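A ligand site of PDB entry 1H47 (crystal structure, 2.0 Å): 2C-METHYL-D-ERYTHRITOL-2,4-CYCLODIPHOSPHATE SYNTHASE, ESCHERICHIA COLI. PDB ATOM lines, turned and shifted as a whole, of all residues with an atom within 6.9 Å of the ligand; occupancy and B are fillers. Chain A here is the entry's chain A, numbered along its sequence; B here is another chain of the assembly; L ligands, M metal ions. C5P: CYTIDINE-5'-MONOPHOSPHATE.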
ATOM      1  N   ILE A 100      22.688  -3.771   7.980  1.00  0.00           N
ATOM      2  CA  ILE A 100      23.914  -3.664   8.735  1.00  0.00           C
ATOM      3  C   ILE A 100      25.120  -3.799   7.747  1.00  0.00           C
ATOM      4  O   ILE A 100      25.095  -4.684   6.908  1.00  0.00           O
ATOM      5  CB  ILE A 100      23.984  -4.766   9.811  1.00  0.00           C
ATOM      6  CG1 ILE A 100      22.807  -4.698  10.771  1.00  0.00           C
ATOM      7  CG2 ILE A 100      25.305  -4.724  10.622  1.00  0.00           C
ATOM      8  CD1 ILE A 100      22.523  -6.003  11.468  1.00  0.00           C
ATOM      9  N   ILE A 101      26.125  -2.930   7.885  1.00  0.00           N
ATOM     10  CA  ILE A 101      27.303  -2.870   7.041  1.00  0.00           C
ATOM     11  C   ILE A 101      28.523  -3.127   7.935  1.00  0.00           C
ATOM     12  O   ILE A 101      28.897  -2.281   8.768  1.00  0.00           O
ATOM     13  CB  ILE A 101      27.367  -1.488   6.356  1.00  0.00           C
ATOM     14  CG1 ILE A 101      26.048  -1.231   5.606  1.00  0.00           C
ATOM     15  CG2 ILE A 101      28.502  -1.428   5.361  1.00  0.00           C
ATOM     16  CD1 ILE A 101      25.887   0.144   5.082  1.00  0.00           C
ATOM     17  N   ALA A 102      29.076  -4.324   7.847  1.00  0.00           N
ATOM     18  CA  ALA A 102      30.098  -4.774   8.769  1.00  0.00           C
ATOM     19  C   ALA A 102      30.905  -5.863   8.121  1.00  0.00           C
ATOM     20  O   ALA A 102      30.350  -6.775   7.507  1.00  0.00           O
ATOM     21  CB  ALA A 102      29.492  -5.270  10.053  1.00  0.00           C
ATOM     22  N   GLN A 103      32.212  -5.727   8.231  1.00  0.00           N
ATOM     23  CA  GLN A 103      33.125  -6.702   7.689  1.00  0.00           C
ATOM     24  C   GLN A 103      33.035  -7.958   8.526  1.00  0.00           C
ATOM     25  O   GLN A 103      33.053  -9.068   8.013  1.00  0.00           O
ATOM     26  CB  GLN A 103      34.557  -6.145   7.714  1.00  0.00           C
ATOM     27  CG  GLN A 103      35.558  -6.927   6.869  1.00  0.00           C
ATOM     28  CD  GLN A 103      35.245  -6.954   5.424  1.00  0.00           C
ATOM     29  OE1 GLN A 103      34.917  -5.938   4.815  1.00  0.00           O
ATOM     30  NE2 GLN A 103      35.352  -8.127   4.834  1.00  0.00           N
ATOM     31  N   ALA A 104      32.896  -7.745   9.830  1.00  0.00           N
ATOM     32  CA  ALA A 104      32.772  -8.787  10.841  1.00  0.00           C
ATOM     33  C   ALA A 104      32.200  -8.118  12.089  1.00  0.00           C
ATOM     34  O   ALA A 104      32.273  -6.883  12.195  1.00  0.00           O
ATOM     35  CB  ALA A 104      34.152  -9.372  11.154  1.00  0.00           C
ATOM     36  N   PRO A 105      31.605  -8.866  13.020  1.00  0.00           N
ATOM     37  CA  PRO A 105      31.400 -10.309  12.913  1.00  0.00           C
ATOM     38  C   PRO A 105      30.289 -10.685  11.956  1.00  0.00           C
ATOM     39  O   PRO A 105      29.637  -9.800  11.374  1.00  0.00           O
ATOM     40  CB  PRO A 105      31.057 -10.722  14.351  1.00  0.00           C
ATOM     41  CG  PRO A 105      30.553  -9.475  15.021  1.00  0.00           C
ATOM     42  CD  PRO A 105      31.088  -8.304  14.276  1.00  0.00           C
ATOM     43  N   LYS A 106      30.108 -11.984  11.736  1.00  0.00           N
ATOM     44  CA  LYS A 106      29.064 -12.469  10.890  1.00  0.00           C
ATOM     45  C   LYS A 106      27.767 -12.204  11.672  1.00  0.00           C
ATOM     46  O   LYS A 106      27.665 -12.478  12.876  1.00  0.00           O
ATOM     47  CB  LYS A 106      29.251 -13.954  10.560  1.00  0.00           C
ATOM     48  CG  LYS A 106      28.239 -14.514   9.566  1.00  0.00           C
ATOM     49  CD  LYS A 106      28.875 -15.138   8.290  1.00  0.00           C
ATOM     50  CE  LYS A 106      28.737 -14.237   7.042  1.00  0.00           C
ATOM     51  NZ  LYS A 106      29.531 -12.939   7.144  1.00  0.00           N
ATOM     52  N   MET A 107      26.809 -11.625  10.970  1.00  0.00           N
ATOM     53  CA  MET A 107      25.562 -11.173  11.595  1.00  0.00           C
ATOM     54  C   MET A 107      24.463 -12.210  11.515  1.00  0.00           C
ATOM     55  O   MET A 107      23.667 -12.268  12.441  1.00  0.00           O
ATOM     56  CB  MET A 107      25.073  -9.876  10.945  1.00  0.00           C
ATOM     57  CG  MET A 107      25.996  -8.693  11.210  1.00  0.00           C
ATOM     58  SD  MET A 107      25.995  -8.230  12.896  1.00  0.00           S
ATOM     59  CE  MET A 107      27.482  -7.262  13.047  1.00  0.00           C
ATOM     60  N   LEU A 108      24.387 -12.982  10.435  1.00  0.00           N
ATOM     61  CA  LEU A 108      23.126 -13.692  10.091  1.00  0.00           C
ATOM     62  C   LEU A 108      22.613 -14.698  11.152  1.00  0.00           C
ATOM     63  O   LEU A 108      21.433 -14.823  11.280  1.00  0.00           O
ATOM     64  CB  LEU A 108      23.144 -14.311   8.689  1.00  0.00           C
ATOM     65  CG  LEU A 108      21.875 -15.038   8.180  1.00  0.00           C
ATOM     66  CD1 LEU A 108      20.759 -14.042   7.696  1.00  0.00           C
ATOM     67  CD2 LEU A 108      22.215 -15.984   7.051  1.00  0.00           C
ATOM     68  N   PRO A 109      23.474 -15.385  11.913  1.00  0.00           N
ATOM     69  CA  PRO A 109      23.000 -16.210  13.037  1.00  0.00           C
ATOM     70  C   PRO A 109      22.328 -15.465  14.198  1.00  0.00           C
ATOM     71  O   PRO A 109      21.683 -16.114  15.042  1.00  0.00           O
ATOM     72  CB  PRO A 109      24.257 -16.907  13.547  1.00  0.00           C
ATOM     73  CG  PRO A 109      25.399 -16.154  12.954  1.00  0.00           C
ATOM     74  CD  PRO A 109      24.924 -15.563  11.693  1.00  0.00           C
ATOM     75  N   ILE A 111      20.524 -12.582  13.505  1.00  0.00           N
ATOM     76  CA  ILE A 111      19.514 -11.787  12.852  1.00  0.00           C
ATOM     77  C   ILE A 111      18.089 -12.212  13.230  1.00  0.00           C
ATOM     78  O   ILE A 111      17.294 -11.344  13.505  1.00  0.00           O
ATOM     79  CB  ILE A 111      19.754 -11.728  11.311  1.00  0.00           C
ATOM     80  CG1 ILE A 111      20.801 -10.626  11.006  1.00  0.00           C
ATOM     81  CG2 ILE A 111      18.490 -11.437  10.531  1.00  0.00           C
ATOM     82  CD1 ILE A 111      21.183 -10.521   9.565  1.00  0.00           C
ATOM     83  N   LYS A 132      19.105  -7.402   7.413  1.00  0.00           N
ATOM     84  CA  LYS A 132      20.170  -8.063   6.676  1.00  0.00           C
ATOM     85  C   LYS A 132      21.517  -7.427   6.963  1.00  0.00           C
ATOM     86  O   LYS A 132      21.618  -6.403   7.627  1.00  0.00           O
ATOM     87  CB  LYS A 132      19.926  -8.084   5.183  1.00  0.00           C
ATOM     88  CG  LYS A 132      19.886  -6.778   4.476  1.00  0.00           C
ATOM     89  CD  LYS A 132      18.545  -6.732   3.694  1.00  0.00           C
ATOM     90  CE  LYS A 132      18.380  -5.570   2.826  1.00  0.00           C
ATOM     91  NZ  LYS A 132      17.682  -4.546   3.563  1.00  0.00           N
ATOM     92  N   ALA A 133      22.562  -8.073   6.436  1.00  0.00           N
ATOM     93  CA  ALA A 133      23.918  -7.574   6.608  1.00  0.00           C
ATOM     94  C   ALA A 133      24.716  -7.738   5.308  1.00  0.00           C
ATOM     95  O   ALA A 133      24.366  -8.540   4.389  1.00  0.00           O
ATOM     96  CB  ALA A 133      24.571  -8.261   7.717  1.00  0.00           C
ATOM     97  N   THR A 134      25.721  -6.893   5.190  1.00  0.00           N
ATOM     98  CA  THR A 134      26.614  -6.934   4.055  1.00  0.00           C
ATOM     99  C   THR A 134      27.971  -6.350   4.464  1.00  0.00           C
ATOM    100  O   THR A 134      28.027  -5.515   5.368  1.00  0.00           O
ATOM    101  CB  THR A 134      25.997  -6.194   2.904  1.00  0.00           C
ATOM    102  OG1 THR A 134      26.763  -6.422   1.738  1.00  0.00           O
ATOM    103  CG2 THR A 134      26.012  -4.694   3.079  1.00  0.00           C
ATOM    104  N   THR A 135      29.024  -6.802   3.782  1.00  0.00           N
ATOM    105  CA  THR A 135      30.372  -6.223   3.925  1.00  0.00           C
ATOM    106  C   THR A 135      30.590  -5.243   2.818  1.00  0.00           C
ATOM    107  O   THR A 135      29.777  -5.132   1.914  1.00  0.00           O
ATOM    108  CB  THR A 135      31.475  -7.296   3.802  1.00  0.00           C
ATOM    109  OG1 THR A 135      31.547  -7.732   2.437  1.00  0.00           O
ATOM    110  CG2 THR A 135      31.153  -8.525   4.566  1.00  0.00           C
ATOM    111  N   THR A 136      31.702  -4.517   2.920  1.00  0.00           N
ATOM    112  CA  THR A 136      32.202  -3.672   1.872  1.00  0.00           C
ATOM    113  C   THR A 136      33.499  -4.243   1.335  1.00  0.00           C
ATOM    114  O   THR A 136      34.389  -3.489   0.938  1.00  0.00           O
ATOM    115  CB  THR A 136      32.485  -2.253   2.371  1.00  0.00           C
ATOM    116  OG1 THR A 136      33.441  -2.300   3.467  1.00  0.00           O
ATOM    117  CG2 THR A 136      31.195  -1.601   2.902  1.00  0.00           C
ATOM    118  N   GLU A 137      33.643  -5.569   1.399  1.00  0.00           N
ATOM    119  CA  GLU A 137      34.701  -6.301   0.720  1.00  0.00           C
ATOM    120  C   GLU A 137      36.085  -5.724   1.042  1.00  0.00           C
ATOM    121  O   GLU A 137      36.875  -5.486   0.151  1.00  0.00           O
ATOM    122  CB  GLU A 137      34.464  -6.242  -0.779  1.00  0.00           C
ATOM    123  CG  GLU A 137      33.099  -6.735  -1.228  1.00  0.00           C
ATOM    124  CD  GLU A 137      32.945  -8.239  -1.155  1.00  0.00           C
ATOM    125  OE1 GLU A 137      31.889  -8.755  -1.556  1.00  0.00           O
ATOM    126  OE2 GLU A 137      33.855  -8.917  -0.649  1.00  0.00           O
ATOM    127  N   ASP B  10      25.240  -2.591  -1.660  1.00  0.00           N
ATOM    128  CA  ASP B  10      26.256  -3.553  -2.050  1.00  0.00           C
ATOM    129  C   ASP B  10      27.514  -2.846  -2.491  1.00  0.00           C
ATOM    130  O   ASP B  10      27.459  -1.698  -2.911  1.00  0.00           O
ATOM    131  CB  ASP B  10      25.771  -4.429  -3.200  1.00  0.00           C
ATOM    132  CG  ASP B  10      26.527  -5.703  -3.314  1.00  0.00           C
ATOM    133  OD1 ASP B  10      27.110  -6.211  -2.324  1.00  0.00           O
ATOM    134  OD2 ASP B  10      26.668  -6.241  -4.425  1.00  0.00           O
ATOM    135  N   VAL B  11      28.617  -3.553  -2.397  1.00  0.00           N
ATOM    136  CA  VAL B  11      29.933  -3.006  -2.720  1.00  0.00           C
ATOM    137  C   VAL B  11      30.717  -4.138  -3.292  1.00  0.00           C
ATOM    138  O   VAL B  11      30.698  -5.233  -2.762  1.00  0.00           O
ATOM    139  CB  VAL B  11      30.661  -2.519  -1.446  1.00  0.00           C
ATOM    140  CG1 VAL B  11      32.179  -2.200  -1.748  1.00  0.00           C
ATOM    141  CG2 VAL B  11      30.000  -1.320  -0.848  1.00  0.00           C
ATOM    142  N   HIS B  12      31.422  -3.891  -4.382  1.00  0.00           N
ATOM    143  CA  HIS B  12      32.550  -4.765  -4.799  1.00  0.00           C
ATOM    144  C   HIS B  12      33.816  -3.981  -5.093  1.00  0.00           C
ATOM    145  O   HIS B  12      33.761  -2.872  -5.555  1.00  0.00           O
ATOM    146  CB  HIS B  12      32.138  -5.595  -6.025  1.00  0.00           C
ATOM    147  CG  HIS B  12      31.217  -6.700  -5.687  1.00  0.00           C
ATOM    148  ND1 HIS B  12      31.602  -7.776  -4.927  1.00  0.00           N
ATOM    149  CD2 HIS B  12      29.881  -6.817  -5.862  1.00  0.00           C
ATOM    150  CE1 HIS B  12      30.560  -8.545  -4.692  1.00  0.00           C
ATOM    151  NE2 HIS B  12      29.505  -7.985  -5.260  1.00  0.00           N
ATOM    152  N   HIS B  44      22.530  -6.567  -7.328  1.00  0.00           N
ATOM    153  CA  HIS B  44      22.570  -7.195  -6.018  1.00  0.00           C
ATOM    154  C   HIS B  44      21.886  -6.297  -4.997  1.00  0.00           C
ATOM    155  O   HIS B  44      21.097  -6.753  -4.204  1.00  0.00           O
ATOM    156  CB  HIS B  44      24.040  -7.506  -5.617  1.00  0.00           C
ATOM    157  CG  HIS B  44      24.658  -8.582  -6.453  1.00  0.00           C
ATOM    158  ND1 HIS B  44      25.954  -9.019  -6.273  1.00  0.00           N
ATOM    159  CD2 HIS B  44      24.164  -9.290  -7.497  1.00  0.00           C
ATOM    160  CE1 HIS B  44      26.227  -9.955  -7.159  1.00  0.00           C
ATOM    161  NE2 HIS B  44      25.168 -10.132  -7.916  1.00  0.00           N
ATOM    162  N   ASP B  48      18.320  -7.066  -3.081  1.00  0.00           N
ATOM    163  CA  ASP B  48      18.212  -6.994  -1.633  1.00  0.00           C
ATOM    164  C   ASP B  48      17.112  -6.058  -1.219  1.00  0.00           C
ATOM    165  O   ASP B  48      16.421  -6.362  -0.240  1.00  0.00           O
ATOM    166  CB  ASP B  48      19.524  -6.539  -0.951  1.00  0.00           C
ATOM    167  CG  ASP B  48      20.466  -7.672  -0.638  1.00  0.00           C
ATOM    168  OD1 ASP B  48      20.126  -8.840  -0.864  1.00  0.00           O
ATOM    169  OD2 ASP B  48      21.597  -7.494  -0.153  1.00  0.00           O
ATOM    170  N   ASP B  58      17.775 -11.581   2.479  1.00  0.00           N
ATOM    171  CA  ASP B  58      18.716 -10.993   1.546  1.00  0.00           C
ATOM    172  C   ASP B  58      19.222 -12.032   0.538  1.00  0.00           C
ATOM    173  O   ASP B  58      18.908 -13.196   0.653  1.00  0.00           O
ATOM    174  CB  ASP B  58      19.880 -10.267   2.280  1.00  0.00           C
ATOM    175  CG  ASP B  58      20.829 -11.199   3.029  1.00  0.00           C
ATOM    176  OD1 ASP B  58      20.786 -12.420   2.868  1.00  0.00           O
ATOM    177  OD2 ASP B  58      21.682 -10.784   3.836  1.00  0.00           O
ATOM    178  N   ILE B  59      20.010 -11.583  -0.408  1.00  0.00           N
ATOM    179  CA  ILE B  59      20.554 -12.418  -1.463  1.00  0.00           C
ATOM    180  C   ILE B  59      21.375 -13.623  -0.921  1.00  0.00           C
ATOM    181  O   ILE B  59      21.297 -14.698  -1.481  1.00  0.00           O
ATOM    182  CB  ILE B  59      21.329 -11.498  -2.426  1.00  0.00           C
ATOM    183  CG1 ILE B  59      21.533 -12.137  -3.784  1.00  0.00           C
ATOM    184  CG2 ILE B  59      22.667 -11.011  -1.779  1.00  0.00           C
ATOM    185  CD1 ILE B  59      21.844 -11.133  -4.852  1.00  0.00           C
ATOM    186  N   GLY B  60      22.104 -13.473   0.180  1.00  0.00           N
ATOM    187  CA  GLY B  60      22.844 -14.583   0.741  1.00  0.00           C
ATOM    188  C   GLY B  60      21.972 -15.633   1.396  1.00  0.00           C
ATOM    189  O   GLY B  60      22.210 -16.848   1.257  1.00  0.00           O
ATOM    190  N   LYS B  61      20.920 -15.190   2.077  1.00  0.00           N
ATOM    191  CA  LYS B  61      19.930 -16.094   2.613  1.00  0.00           C
ATOM    192  C   LYS B  61      19.212 -16.885   1.534  1.00  0.00           C
ATOM    193  O   LYS B  61      18.967 -18.066   1.722  1.00  0.00           O
ATOM    194  CB  LYS B  61      18.911 -15.342   3.453  1.00  0.00           C
ATOM    195  CG  LYS B  61      17.835 -16.233   4.064  1.00  0.00           C
ATOM    196  CD  LYS B  61      17.392 -15.739   5.433  1.00  0.00           C
ATOM    197  CE  LYS B  61      16.277 -16.570   6.019  1.00  0.00           C
ATOM    198  NZ  LYS B  61      15.076 -15.717   6.288  1.00  0.00           N
HETATM  199  O3P C5P L   1      29.334  -8.611   1.682  1.00  0.00           O
HETATM  200  P   C5P L   1      28.957 -10.056   1.196  1.00  0.00           P
HETATM  201  O1P C5P L   1      28.434 -10.024  -0.287  1.00  0.00           O
HETATM  202  O2P C5P L   1      30.168 -11.069   1.401  1.00  0.00           O
HETATM  203  O5' C5P L   1      27.765 -10.618   2.051  1.00  0.00           O
HETATM  204  C5' C5P L   1      27.417 -11.934   1.696  1.00  0.00           C
HETATM  205  C4' C5P L   1      26.413 -12.437   2.670  1.00  0.00           C
HETATM  206  O4' C5P L   1      26.858 -12.720   3.998  1.00  0.00           O
HETATM  207  C3' C5P L   1      25.177 -11.551   2.741  1.00  0.00           C
HETATM  208  O3' C5P L   1      24.181 -11.829   1.739  1.00  0.00           O
HETATM  209  C2' C5P L   1      24.799 -11.616   4.205  1.00  0.00           C
HETATM  210  O2' C5P L   1      23.730 -12.531   4.145  1.00  0.00           O
HETATM  211  C1' C5P L   1      25.926 -12.268   5.007  1.00  0.00           C
HETATM  212  N1  C5P L   1      26.652 -11.373   5.959  1.00  0.00           N
HETATM  213  C2  C5P L   1      26.628 -11.566   7.364  1.00  0.00           C
HETATM  214  N3  C5P L   1      27.346 -10.779   8.178  1.00  0.00           N
HETATM  215  C4  C5P L   1      28.070  -9.762   7.667  1.00  0.00           C
HETATM  216  C5  C5P L   1      28.114  -9.549   6.308  1.00  0.00           C
HETATM  217  C6  C5P L   1      27.403 -10.385   5.473  1.00  0.00           C
HETATM  218  O2  C5P L   1      25.960 -12.490   7.878  1.00  0.00           O
HETATM  219  N4  C5P L   1      28.785  -8.966   8.491  1.00  0.00           N
HETATM  220 ZN    ZN M   1      27.179  -8.029  -4.653  1.00  0.00          ZN
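OG1 of Thr 135 is in hydrogen-bond range of N of Glu 137, 3.2 Å away. The side-chain carboxylate of Asp 58 of chain B lies within hydrogen-bond range of the backbone NH of Gly 60 of chain B, 3.2 Å away. N of Lys 61 of chain B sits at hydrogen-bond distance from OD1 of Asp 58 of chain B (2.9 Å). O of Thr 134 is in hydrogen-bond range of N of Ala 102 (2.9 Å). N of Thr 134 sits at hydrogen-bond distance from O of Ile 100 (2.9 Å). The backbone NH (N) of Ile 59 of chain B lies within hydrogen-bond range of the side-chain carboxylate (OD1) of Asp 48 of chain B, at 2.8 Å.
O3P of the ligand is in hydrogen-bond range of N of Thr 135, 2.8 Å away. The side-chain hydroxyl (OG1) of Thr 135 is in hydrogen-bond range of an oxygen (O3P) of the ligand, at 2.5 Å. An oxygen (O2') of the ligand lies within hydrogen-bond range of the side-chain carboxylate (OD2) of Asp 58 of chain B (2.7 Å). A nitrogen (N4) of the ligand sits at hydrogen-bond distance from the backbone carbonyl oxygen (O) of Ala 102, at 2.9 Å. N of Met 107 is in hydrogen-bond range of N3 of the ligand (3.0 Å). The backbone NH of Leu 108 is in hydrogen-bond range of an oxygen (O2) of the ligand (3.0 Å). The backbone NH (N) of Gly 60 of chain B lies within hydrogen-bond range of an oxygen (O3') of the ligand. The backbone carbonyl oxygen (O) of Pro 105 sits at hydrogen-bond distance from a nitrogen (N4) of the ligand. A nitrogen (N3) of the ligand lies close to the side-chain amino group (NZ) of Lys 106, 3.2 Å away. O3P of the ligand is in hydrogen-bond range of OG1 of Thr 134 (3.4 Å).
Ala 133 touches the ligand. Glu 137 touches the ligand (OE1 to O1P, 3.9 Å). Ile 59 of chain B touches the ligand (CG2 to O3', 3.9 Å). Hydrophobic or aromatic side chains within 4 Å of the ligand: Met 107, Leu 108, Ala 133 and Ile 59 of chain B. 12 residues have an atom within 4 Å of the ligand: Ala 102, Pro 105, Lys 106, Met 107, Leu 108, Ala 133, Thr 134, Thr 135, Glu 137, Asp 58 of chain B, Ile 59 of chain B and Gly 60 of chain B. Along chain A the residues within 4 Å of the ligand span positions 102 to 137.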
